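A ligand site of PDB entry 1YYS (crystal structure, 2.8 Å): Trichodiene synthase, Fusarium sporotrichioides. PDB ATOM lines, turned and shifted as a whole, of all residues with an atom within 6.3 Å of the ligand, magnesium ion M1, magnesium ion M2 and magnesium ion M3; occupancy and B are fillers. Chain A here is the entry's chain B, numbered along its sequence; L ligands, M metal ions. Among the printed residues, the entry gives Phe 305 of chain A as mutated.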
ATOM      1  N   LEU A  97     -14.244  -0.338 -12.379  1.00  0.00           N
ATOM      2  CA  LEU A  97     -15.412   0.401 -12.846  1.00  0.00           C
ATOM      3  C   LEU A  97     -15.065   1.774 -13.381  1.00  0.00           C
ATOM      4  O   LEU A  97     -15.692   2.251 -14.335  1.00  0.00           O
ATOM      5  CB  LEU A  97     -16.431   0.559 -11.718  1.00  0.00           C
ATOM      6  CG  LEU A  97     -17.699   1.278 -12.184  1.00  0.00           C
ATOM      7  CD1 LEU A  97     -18.325   0.473 -13.301  1.00  0.00           C
ATOM      8  CD2 LEU A  97     -18.670   1.462 -11.033  1.00  0.00           C
ATOM      9  N   ASP A 100     -14.112   1.148 -16.816  1.00  0.00           N
ATOM     10  CA  ASP A 100     -15.237   0.668 -17.619  1.00  0.00           C
ATOM     11  C   ASP A 100     -16.088   1.777 -18.206  1.00  0.00           C
ATOM     12  O   ASP A 100     -16.772   1.571 -19.211  1.00  0.00           O
ATOM     13  CB  ASP A 100     -16.124  -0.280 -16.787  1.00  0.00           C
ATOM     14  CG  ASP A 100     -17.237  -0.916 -17.615  1.00  0.00           C
ATOM     15  OD1 ASP A 100     -18.211  -0.213 -17.954  1.00  0.00           O
ATOM     16  OD2 ASP A 100     -17.122  -2.125 -17.949  1.00  0.00           O
ATOM     17  N   ASP A 101     -16.028   2.947 -17.571  1.00  0.00           N
ATOM     18  CA  ASP A 101     -16.792   4.092 -18.039  1.00  0.00           C
ATOM     19  C   ASP A 101     -15.896   5.175 -18.654  1.00  0.00           C
ATOM     20  O   ASP A 101     -16.383   6.258 -18.990  1.00  0.00           O
ATOM     21  CB  ASP A 101     -17.633   4.694 -16.885  1.00  0.00           C
ATOM     22  CG  ASP A 101     -18.727   3.741 -16.377  1.00  0.00           C
ATOM     23  OD1 ASP A 101     -19.371   3.049 -17.192  1.00  0.00           O
ATOM     24  OD2 ASP A 101     -18.946   3.690 -15.139  1.00  0.00           O
ATOM     25  N   PHE A 157      -9.981  -7.684 -18.703  1.00  0.00           N
ATOM     26  CA  PHE A 157     -10.816  -6.501 -18.563  1.00  0.00           C
ATOM     27  C   PHE A 157     -10.167  -5.264 -19.192  1.00  0.00           C
ATOM     28  O   PHE A 157     -10.863  -4.458 -19.831  1.00  0.00           O
ATOM     29  CB  PHE A 157     -11.107  -6.240 -17.079  1.00  0.00           C
ATOM     30  CG  PHE A 157     -12.050  -5.114 -16.842  1.00  0.00           C
ATOM     31  CD1 PHE A 157     -13.387  -5.227 -17.220  1.00  0.00           C
ATOM     32  CD2 PHE A 157     -11.599  -3.915 -16.287  1.00  0.00           C
ATOM     33  CE1 PHE A 157     -14.258  -4.158 -17.054  1.00  0.00           C
ATOM     34  CE2 PHE A 157     -12.470  -2.845 -16.110  1.00  0.00           C
ATOM     35  CZ  PHE A 157     -13.794  -2.964 -16.489  1.00  0.00           C
ATOM     36  N   CYS A 161     -11.901  -2.990 -22.157  1.00  0.00           N
ATOM     37  CA  CYS A 161     -12.169  -1.566 -22.207  1.00  0.00           C
ATOM     38  C   CYS A 161     -11.536  -0.972 -23.472  1.00  0.00           C
ATOM     39  O   CYS A 161     -12.099  -0.084 -24.122  1.00  0.00           O
ATOM     40  CB  CYS A 161     -11.605  -0.885 -20.959  1.00  0.00           C
ATOM     41  SG  CYS A 161     -12.478  -1.387 -19.460  1.00  0.00           S
ATOM     42  N   GLU A 164     -13.727  -1.703 -26.340  1.00  0.00           N
ATOM     43  CA  GLU A 164     -14.953  -0.927 -26.261  1.00  0.00           C
ATOM     44  C   GLU A 164     -14.769   0.522 -26.668  1.00  0.00           C
ATOM     45  O   GLU A 164     -15.736   1.183 -27.044  1.00  0.00           O
ATOM     46  CB  GLU A 164     -15.553  -1.008 -24.863  1.00  0.00           C
ATOM     47  CG  GLU A 164     -15.952  -2.409 -24.471  1.00  0.00           C
ATOM     48  CD  GLU A 164     -17.070  -2.426 -23.456  1.00  0.00           C
ATOM     49  OE1 GLU A 164     -16.939  -1.776 -22.388  1.00  0.00           O
ATOM     50  OE2 GLU A 164     -18.090  -3.105 -23.732  1.00  0.00           O
ATOM     51  N   ARG A 182     -18.189  -9.819 -24.306  1.00  0.00           N
ATOM     52  CA  ARG A 182     -18.798  -9.793 -22.980  1.00  0.00           C
ATOM     53  C   ARG A 182     -17.887 -10.461 -21.971  1.00  0.00           C
ATOM     54  O   ARG A 182     -17.750  -9.983 -20.844  1.00  0.00           O
ATOM     55  CB  ARG A 182     -20.158 -10.492 -22.999  1.00  0.00           C
ATOM     56  CG  ARG A 182     -20.918 -10.387 -21.688  1.00  0.00           C
ATOM     57  CD  ARG A 182     -20.886  -8.980 -21.137  1.00  0.00           C
ATOM     58  NE  ARG A 182     -21.841  -8.807 -20.057  1.00  0.00           N
ATOM     59  CZ  ARG A 182     -21.784  -7.837 -19.157  1.00  0.00           C
ATOM     60  NH1 ARG A 182     -20.817  -6.938 -19.214  1.00  0.00           N
ATOM     61  NH2 ARG A 182     -22.707  -7.758 -18.201  1.00  0.00           N
ATOM     62  N   ASN A 185     -14.740  -8.152 -21.090  1.00  0.00           N
ATOM     63  CA  ASN A 185     -14.966  -7.036 -20.180  1.00  0.00           C
ATOM     64  C   ASN A 185     -15.844  -7.396 -18.979  1.00  0.00           C
ATOM     65  O   ASN A 185     -16.228  -6.519 -18.220  1.00  0.00           O
ATOM     66  CB  ASN A 185     -15.620  -5.893 -20.951  1.00  0.00           C
ATOM     67  CG  ASN A 185     -17.114  -6.088 -21.104  1.00  0.00           C
ATOM     68  OD1 ASN A 185     -17.603  -7.221 -21.218  1.00  0.00           O
ATOM     69  ND2 ASN A 185     -17.859  -4.983 -21.095  1.00  0.00           N
ATOM     70  N   GLY A 186     -16.139  -8.679 -18.822  1.00  0.00           N
ATOM     71  CA  GLY A 186     -16.998  -9.116 -17.735  1.00  0.00           C
ATOM     72  C   GLY A 186     -16.410  -9.392 -16.365  1.00  0.00           C
ATOM     73  O   GLY A 186     -17.154  -9.446 -15.391  1.00  0.00           O
ATOM     74  N   VAL A 222     -22.426 -12.306 -15.591  1.00  0.00           N
ATOM     75  CA  VAL A 222     -22.552 -11.298 -16.659  1.00  0.00           C
ATOM     76  C   VAL A 222     -23.922 -11.246 -17.335  1.00  0.00           C
ATOM     77  O   VAL A 222     -24.406 -10.173 -17.670  1.00  0.00           O
ATOM     78  CB  VAL A 222     -21.481 -11.480 -17.759  1.00  0.00           C
ATOM     79  CG1 VAL A 222     -20.107 -11.327 -17.155  1.00  0.00           C
ATOM     80  CG2 VAL A 222     -21.646 -12.811 -18.437  1.00  0.00           C
ATOM     81  N   ASN A 225     -26.429  -9.531 -15.198  1.00  0.00           N
ATOM     82  CA  ASN A 225     -26.221  -8.089 -15.263  1.00  0.00           C
ATOM     83  C   ASN A 225     -26.723  -7.520 -16.592  1.00  0.00           C
ATOM     84  O   ASN A 225     -27.307  -6.443 -16.625  1.00  0.00           O
ATOM     85  CB  ASN A 225     -24.751  -7.731 -15.085  1.00  0.00           C
ATOM     86  CG  ASN A 225     -24.458  -6.276 -15.442  1.00  0.00           C
ATOM     87  OD1 ASN A 225     -24.228  -5.943 -16.601  1.00  0.00           O
ATOM     88  ND2 ASN A 225     -24.493  -5.410 -14.442  1.00  0.00           N
ATOM     89  N   ASP A 226     -26.502  -8.233 -17.686  1.00  0.00           N
ATOM     90  CA  ASP A 226     -26.980  -7.727 -18.970  1.00  0.00           C
ATOM     91  C   ASP A 226     -28.497  -7.619 -18.922  1.00  0.00           C
ATOM     92  O   ASP A 226     -29.074  -6.675 -19.466  1.00  0.00           O
ATOM     93  CB  ASP A 226     -26.556  -8.655 -20.120  1.00  0.00           C
ATOM     94  CG  ASP A 226     -25.122  -8.431 -20.551  1.00  0.00           C
ATOM     95  OD1 ASP A 226     -24.725  -7.268 -20.765  1.00  0.00           O
ATOM     96  OD2 ASP A 226     -24.382  -9.433 -20.692  1.00  0.00           O
ATOM     97  N   LEU A 227     -29.139  -8.580 -18.263  1.00  0.00           N
ATOM     98  CA  LEU A 227     -30.591  -8.594 -18.147  1.00  0.00           C
ATOM     99  C   LEU A 227     -31.105  -7.444 -17.284  1.00  0.00           C
ATOM    100  O   LEU A 227     -31.921  -6.649 -17.740  1.00  0.00           O
ATOM    101  CB  LEU A 227     -31.059  -9.926 -17.554  1.00  0.00           C
ATOM    102  CG  LEU A 227     -32.572 -10.122 -17.524  1.00  0.00           C
ATOM    103  CD1 LEU A 227     -33.103 -10.241 -18.946  1.00  0.00           C
ATOM    104  CD2 LEU A 227     -32.921 -11.381 -16.728  1.00  0.00           C
ATOM    105  N   SER A 229     -29.579  -4.830 -16.387  1.00  0.00           N
ATOM    106  CA  SER A 229     -29.155  -3.538 -16.921  1.00  0.00           C
ATOM    107  C   SER A 229     -29.888  -3.163 -18.207  1.00  0.00           C
ATOM    108  O   SER A 229     -29.753  -2.049 -18.694  1.00  0.00           O
ATOM    109  CB  SER A 229     -27.648  -3.544 -17.221  1.00  0.00           C
ATOM    110  OG  SER A 229     -26.865  -3.598 -16.046  1.00  0.00           O
ATOM    111  N   PHE A 230     -30.677  -4.096 -18.739  1.00  0.00           N
ATOM    112  CA  PHE A 230     -31.393  -3.839 -19.994  1.00  0.00           C
ATOM    113  C   PHE A 230     -32.227  -2.559 -19.954  1.00  0.00           C
ATOM    114  O   PHE A 230     -32.798  -2.154 -20.966  1.00  0.00           O
ATOM    115  CB  PHE A 230     -32.219  -5.056 -20.401  1.00  0.00           C
ATOM    116  CG  PHE A 230     -32.823  -4.942 -21.771  1.00  0.00           C
ATOM    117  CD1 PHE A 230     -32.032  -4.601 -22.872  1.00  0.00           C
ATOM    118  CD2 PHE A 230     -34.176  -5.170 -21.964  1.00  0.00           C
ATOM    119  CE1 PHE A 230     -32.592  -4.486 -24.145  1.00  0.00           C
ATOM    120  CE2 PHE A 230     -34.749  -5.049 -23.238  1.00  0.00           C
ATOM    121  CZ  PHE A 230     -33.957  -4.707 -24.328  1.00  0.00           C
ATOM    122  N   LYS A 232     -31.102   0.806 -17.717  1.00  0.00           N
ATOM    123  CA  LYS A 232     -30.111   1.876 -17.683  1.00  0.00           C
ATOM    124  C   LYS A 232     -29.205   2.021 -18.915  1.00  0.00           C
ATOM    125  O   LYS A 232     -28.837   3.141 -19.293  1.00  0.00           O
ATOM    126  CB  LYS A 232     -29.261   1.776 -16.408  1.00  0.00           C
ATOM    127  CG  LYS A 232     -28.106   0.792 -16.459  1.00  0.00           C
ATOM    128  CD  LYS A 232     -26.792   1.489 -16.818  1.00  0.00           C
ATOM    129  CE  LYS A 232     -25.587   0.543 -16.716  1.00  0.00           C
ATOM    130  NZ  LYS A 232     -24.285   1.211 -16.990  1.00  0.00           N
ATOM    131  N   GLU A 233     -28.818   0.903 -19.546  1.00  0.00           N
ATOM    132  CA  GLU A 233     -27.980   0.967 -20.752  1.00  0.00           C
ATOM    133  C   GLU A 233     -28.944   0.998 -21.929  1.00  0.00           C
ATOM    134  O   GLU A 233     -29.822   0.125 -22.025  1.00  0.00           O
ATOM    135  CB  GLU A 233     -27.101  -0.267 -20.922  1.00  0.00           C
ATOM    136  CG  GLU A 233     -26.377  -0.775 -19.681  1.00  0.00           C
ATOM    137  CD  GLU A 233     -25.580  -2.034 -19.972  1.00  0.00           C
ATOM    138  OE1 GLU A 233     -25.170  -2.734 -19.014  1.00  0.00           O
ATOM    139  OE2 GLU A 233     -25.357  -2.334 -21.162  1.00  0.00           O
ATOM    140  N   ARG A 238     -21.935   5.626 -23.406  1.00  0.00           N
ATOM    141  CA  ARG A 238     -20.826   4.678 -23.234  1.00  0.00           C
ATOM    142  C   ARG A 238     -21.315   3.253 -23.448  1.00  0.00           C
ATOM    143  O   ARG A 238     -20.517   2.325 -23.542  1.00  0.00           O
ATOM    144  CB  ARG A 238     -20.189   4.816 -21.844  1.00  0.00           C
ATOM    145  CG  ARG A 238     -19.058   3.810 -21.556  1.00  0.00           C
ATOM    146  CD  ARG A 238     -17.962   3.838 -22.631  1.00  0.00           C
ATOM    147  NE  ARG A 238     -16.794   3.016 -22.276  1.00  0.00           N
ATOM    148  CZ  ARG A 238     -16.765   1.686 -22.245  1.00  0.00           C
ATOM    149  NH1 ARG A 238     -17.851   0.975 -22.532  1.00  0.00           N
ATOM    150  NH2 ARG A 238     -15.652   1.046 -21.905  1.00  0.00           N
ATOM    151  N   SER A 242     -23.723  -3.089 -26.171  1.00  0.00           N
ATOM    152  CA  SER A 242     -23.982  -4.035 -25.095  1.00  0.00           C
ATOM    153  C   SER A 242     -24.133  -5.420 -25.708  1.00  0.00           C
ATOM    154  O   SER A 242     -24.299  -5.547 -26.911  1.00  0.00           O
ATOM    155  CB  SER A 242     -25.250  -3.648 -24.332  1.00  0.00           C
ATOM    156  OG  SER A 242     -26.396  -3.707 -25.159  1.00  0.00           O
ATOM    157  N   TRP A 298     -28.666  -6.291  -5.039  1.00  0.00           N
ATOM    158  CA  TRP A 298     -27.919  -5.109  -5.429  1.00  0.00           C
ATOM    159  C   TRP A 298     -28.487  -4.460  -6.679  1.00  0.00           C
ATOM    160  O   TRP A 298     -28.613  -3.247  -6.759  1.00  0.00           O
ATOM    161  CB  TRP A 298     -26.443  -5.475  -5.658  1.00  0.00           C
ATOM    162  CG  TRP A 298     -25.601  -4.373  -6.230  1.00  0.00           C
ATOM    163  CD1 TRP A 298     -25.316  -3.170  -5.649  1.00  0.00           C
ATOM    164  CD2 TRP A 298     -24.903  -4.387  -7.485  1.00  0.00           C
ATOM    165  NE1 TRP A 298     -24.488  -2.438  -6.462  1.00  0.00           N
ATOM    166  CE2 TRP A 298     -24.218  -3.160  -7.601  1.00  0.00           C
ATOM    167  CE3 TRP A 298     -24.797  -5.330  -8.523  1.00  0.00           C
ATOM    168  CZ2 TRP A 298     -23.432  -2.842  -8.709  1.00  0.00           C
ATOM    169  CZ3 TRP A 298     -24.010  -5.011  -9.631  1.00  0.00           C
ATOM    170  CH2 TRP A 298     -23.345  -3.778  -9.716  1.00  0.00           C
ATOM    171  N   HIS A 299     -28.833  -5.275  -7.670  1.00  0.00           N
ATOM    172  CA  HIS A 299     -29.378  -4.733  -8.911  1.00  0.00           C
ATOM    173  C   HIS A 299     -30.671  -4.004  -8.628  1.00  0.00           C
ATOM    174  O   HIS A 299     -30.861  -2.858  -9.048  1.00  0.00           O
ATOM    175  CB  HIS A 299     -29.610  -5.840  -9.930  1.00  0.00           C
ATOM    176  CG  HIS A 299     -28.361  -6.252 -10.658  1.00  0.00           C
ATOM    177  ND1 HIS A 299     -27.829  -5.502 -11.688  1.00  0.00           N
ATOM    178  CD2 HIS A 299     -27.516  -7.290 -10.462  1.00  0.00           C
ATOM    179  CE1 HIS A 299     -26.714  -6.076 -12.103  1.00  0.00           C
ATOM    180  NE2 HIS A 299     -26.504  -7.160 -11.378  1.00  0.00           N
ATOM    181  N   ARG A 304     -28.607   3.049  -9.849  1.00  0.00           N
ATOM    182  CA  ARG A 304     -27.915   2.905 -11.120  1.00  0.00           C
ATOM    183  C   ARG A 304     -28.759   2.186 -12.176  1.00  0.00           C
ATOM    184  O   ARG A 304     -28.737   2.538 -13.357  1.00  0.00           O
ATOM    185  CB  ARG A 304     -26.621   2.133 -10.903  1.00  0.00           C
ATOM    186  CG  ARG A 304     -25.744   1.986 -12.131  1.00  0.00           C
ATOM    187  CD  ARG A 304     -24.734   0.866 -11.900  1.00  0.00           C
ATOM    188  NE  ARG A 304     -23.614   0.912 -12.828  1.00  0.00           N
ATOM    189  CZ  ARG A 304     -22.777   1.945 -12.937  1.00  0.00           C
ATOM    190  NH1 ARG A 304     -22.957   3.020 -12.178  1.00  0.00           N
ATOM    191  NH2 ARG A 304     -21.757   1.892 -13.804  1.00  0.00           N
ATOM    192  N   PHE A 305     -29.524   1.190 -11.744  1.00  0.00           N
ATOM    193  CA  PHE A 305     -30.336   0.418 -12.665  1.00  0.00           C
ATOM    194  C   PHE A 305     -31.807   0.842 -12.767  1.00  0.00           C
ATOM    195  O   PHE A 305     -32.598   0.151 -13.416  1.00  0.00           O
ATOM    196  CB  PHE A 305     -30.231  -1.061 -12.292  1.00  0.00           C
ATOM    197  CG  PHE A 305     -28.809  -1.518 -12.152  1.00  0.00           C
ATOM    198  CD1 PHE A 305     -28.264  -1.764 -10.893  1.00  0.00           C
ATOM    199  CD2 PHE A 305     -28.002  -1.666 -13.271  1.00  0.00           C
ATOM    200  CE1 PHE A 305     -26.934  -2.155 -10.751  1.00  0.00           C
ATOM    201  CE2 PHE A 305     -26.663  -2.055 -13.141  1.00  0.00           C
ATOM    202  CZ  PHE A 305     -26.138  -2.307 -11.880  1.00  0.00           C
HETATM  203  P1  LIG L   1     -20.609  -4.034 -17.922  1.00  0.00           P
HETATM  204  O1  LIG L   1     -21.694  -4.250 -18.970  1.00  0.00           O
HETATM  205  O2  LIG L   1     -19.551  -3.117 -18.474  1.00  0.00           O
HETATM  206  O3  LIG L   1     -19.970  -5.304 -17.490  1.00  0.00           O
HETATM  207  O4  LIG L   1     -21.418  -3.686 -16.521  1.00  0.00           O
HETATM  208  P2  LIG L   1     -22.410  -2.376 -16.158  1.00  0.00           P
HETATM  209  O5  LIG L   1     -23.653  -2.325 -17.078  1.00  0.00           O
HETATM  210  O6  LIG L   1     -21.543  -1.138 -16.302  1.00  0.00           O
HETATM  211  O7  LIG L   1     -22.786  -2.695 -14.795  1.00  0.00           O
HETATM  212 MG    MG M   1     -24.696  -4.632 -18.599  1.00  0.00          MG
HETATM  213 MG    MG M   2     -20.691  -0.958 -18.472  1.00  0.00          MG
HETATM  214 MG    MG M   3     -18.018  -2.839 -19.919  1.00  0.00          MG
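OG of Ser 229 touches O5 of the ligand (3.6 Å). Eight residues have an atom within 4 Å of the ligand: Asp 100, Arg 182, Asn 185, Asn 225, Ser 229, Lys 232, Glu 233 and Arg 304. The nearest printed residue that does not touch the ligand is Phe 305 (4.3 Å).
Magnesium ion M1 is bound by the side-chain carboxylate of Glu 233 (2.0 Å) and the side-chain amide oxygen of Asn 225 (2.4 Å).
Magnesium ion M3 is bound by an oxygen (O2) of the ligand, the side-chain carboxylate (OD2) of Asp 100 and the side-chain amide nitrogen (ND2) of Asn 185. Magnesium ion M3 has three donor atoms within binding distance.
Merely in contact with magnesium ion M3: Glu 164 (2.9 Å). Of the 23 residues printed, 3 come within 4 Å of magnesium ion M3. The nearest printed residue that does not touch magnesium ion M3 is Arg 238 (4.6 Å).
NH1 of Arg 182 is in salt-bridge range of O3 of the ligand, 2.5 Å away. An oxygen (O6) of the ligand sits close to the guanidinium group (NH2) of Arg 304 (3.9 Å). OE1 of Glu 233 sits close to O5 of the ligand (2.5 Å). ND2 of Asn 225 lies within hydrogen-bond range of O7 of the ligand (3.2 Å). The side-chain amino group (NZ) of Lys 232 lies within salt-bridge range of an oxygen (O5) of the ligand, at 3.6 Å.
Within 4 Å of magnesium ion M2: Asp 100. The nearest printed residue that does not touch magnesium ion M2 is Asp 101 (4.4 Å).
Residues that only touch magnesium ion M1: Asp 226, Ser 229 and Arg 182. The nearest printed residue that does not touch magnesium ion M1 is Lys 232 (5.6 Å).
Magnesium ion M2 is bound by an oxygen (O6) of the ligand and an oxygen (O2) of the ligand. Slightly farther from magnesium ion M2 lies the side-chain carboxylate (OD1) of Asp 100 (2.6 Å).
OE1 of Glu 164 is in salt-bridge range of NH1 of Arg 238. The side-chain amide oxygen (OD1) of Asn 225 sits close to the guanidinium group (NH2) of Arg 182 (2.9 Å). The backbone carbonyl oxygen of Asp 100 sits at hydrogen-bond distance from the guanidinium group of Arg 238 (3.0 Å). O of Asn 225 is in hydrogen-bond range of OG of Ser 229 (2.9 Å). The guanidinium group (NH2) of Arg 304 lies within salt-bridge range of the side-chain carboxylate (OD2) of Asp 101, 3.6 Å away. The backbone carbonyl oxygen (O) of Arg 182 lies close to the side-chain amide oxygen (OD1) of Asn 185 (2.8 Å). The backbone carbonyl oxygen (O) of Val 222 lies within hydrogen-bond range of the guanidinium group (NH2) of Arg 182 (3.0 Å). ND2 of Asn 185 lies close to OE2 of Glu 164 (3.2 Å).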
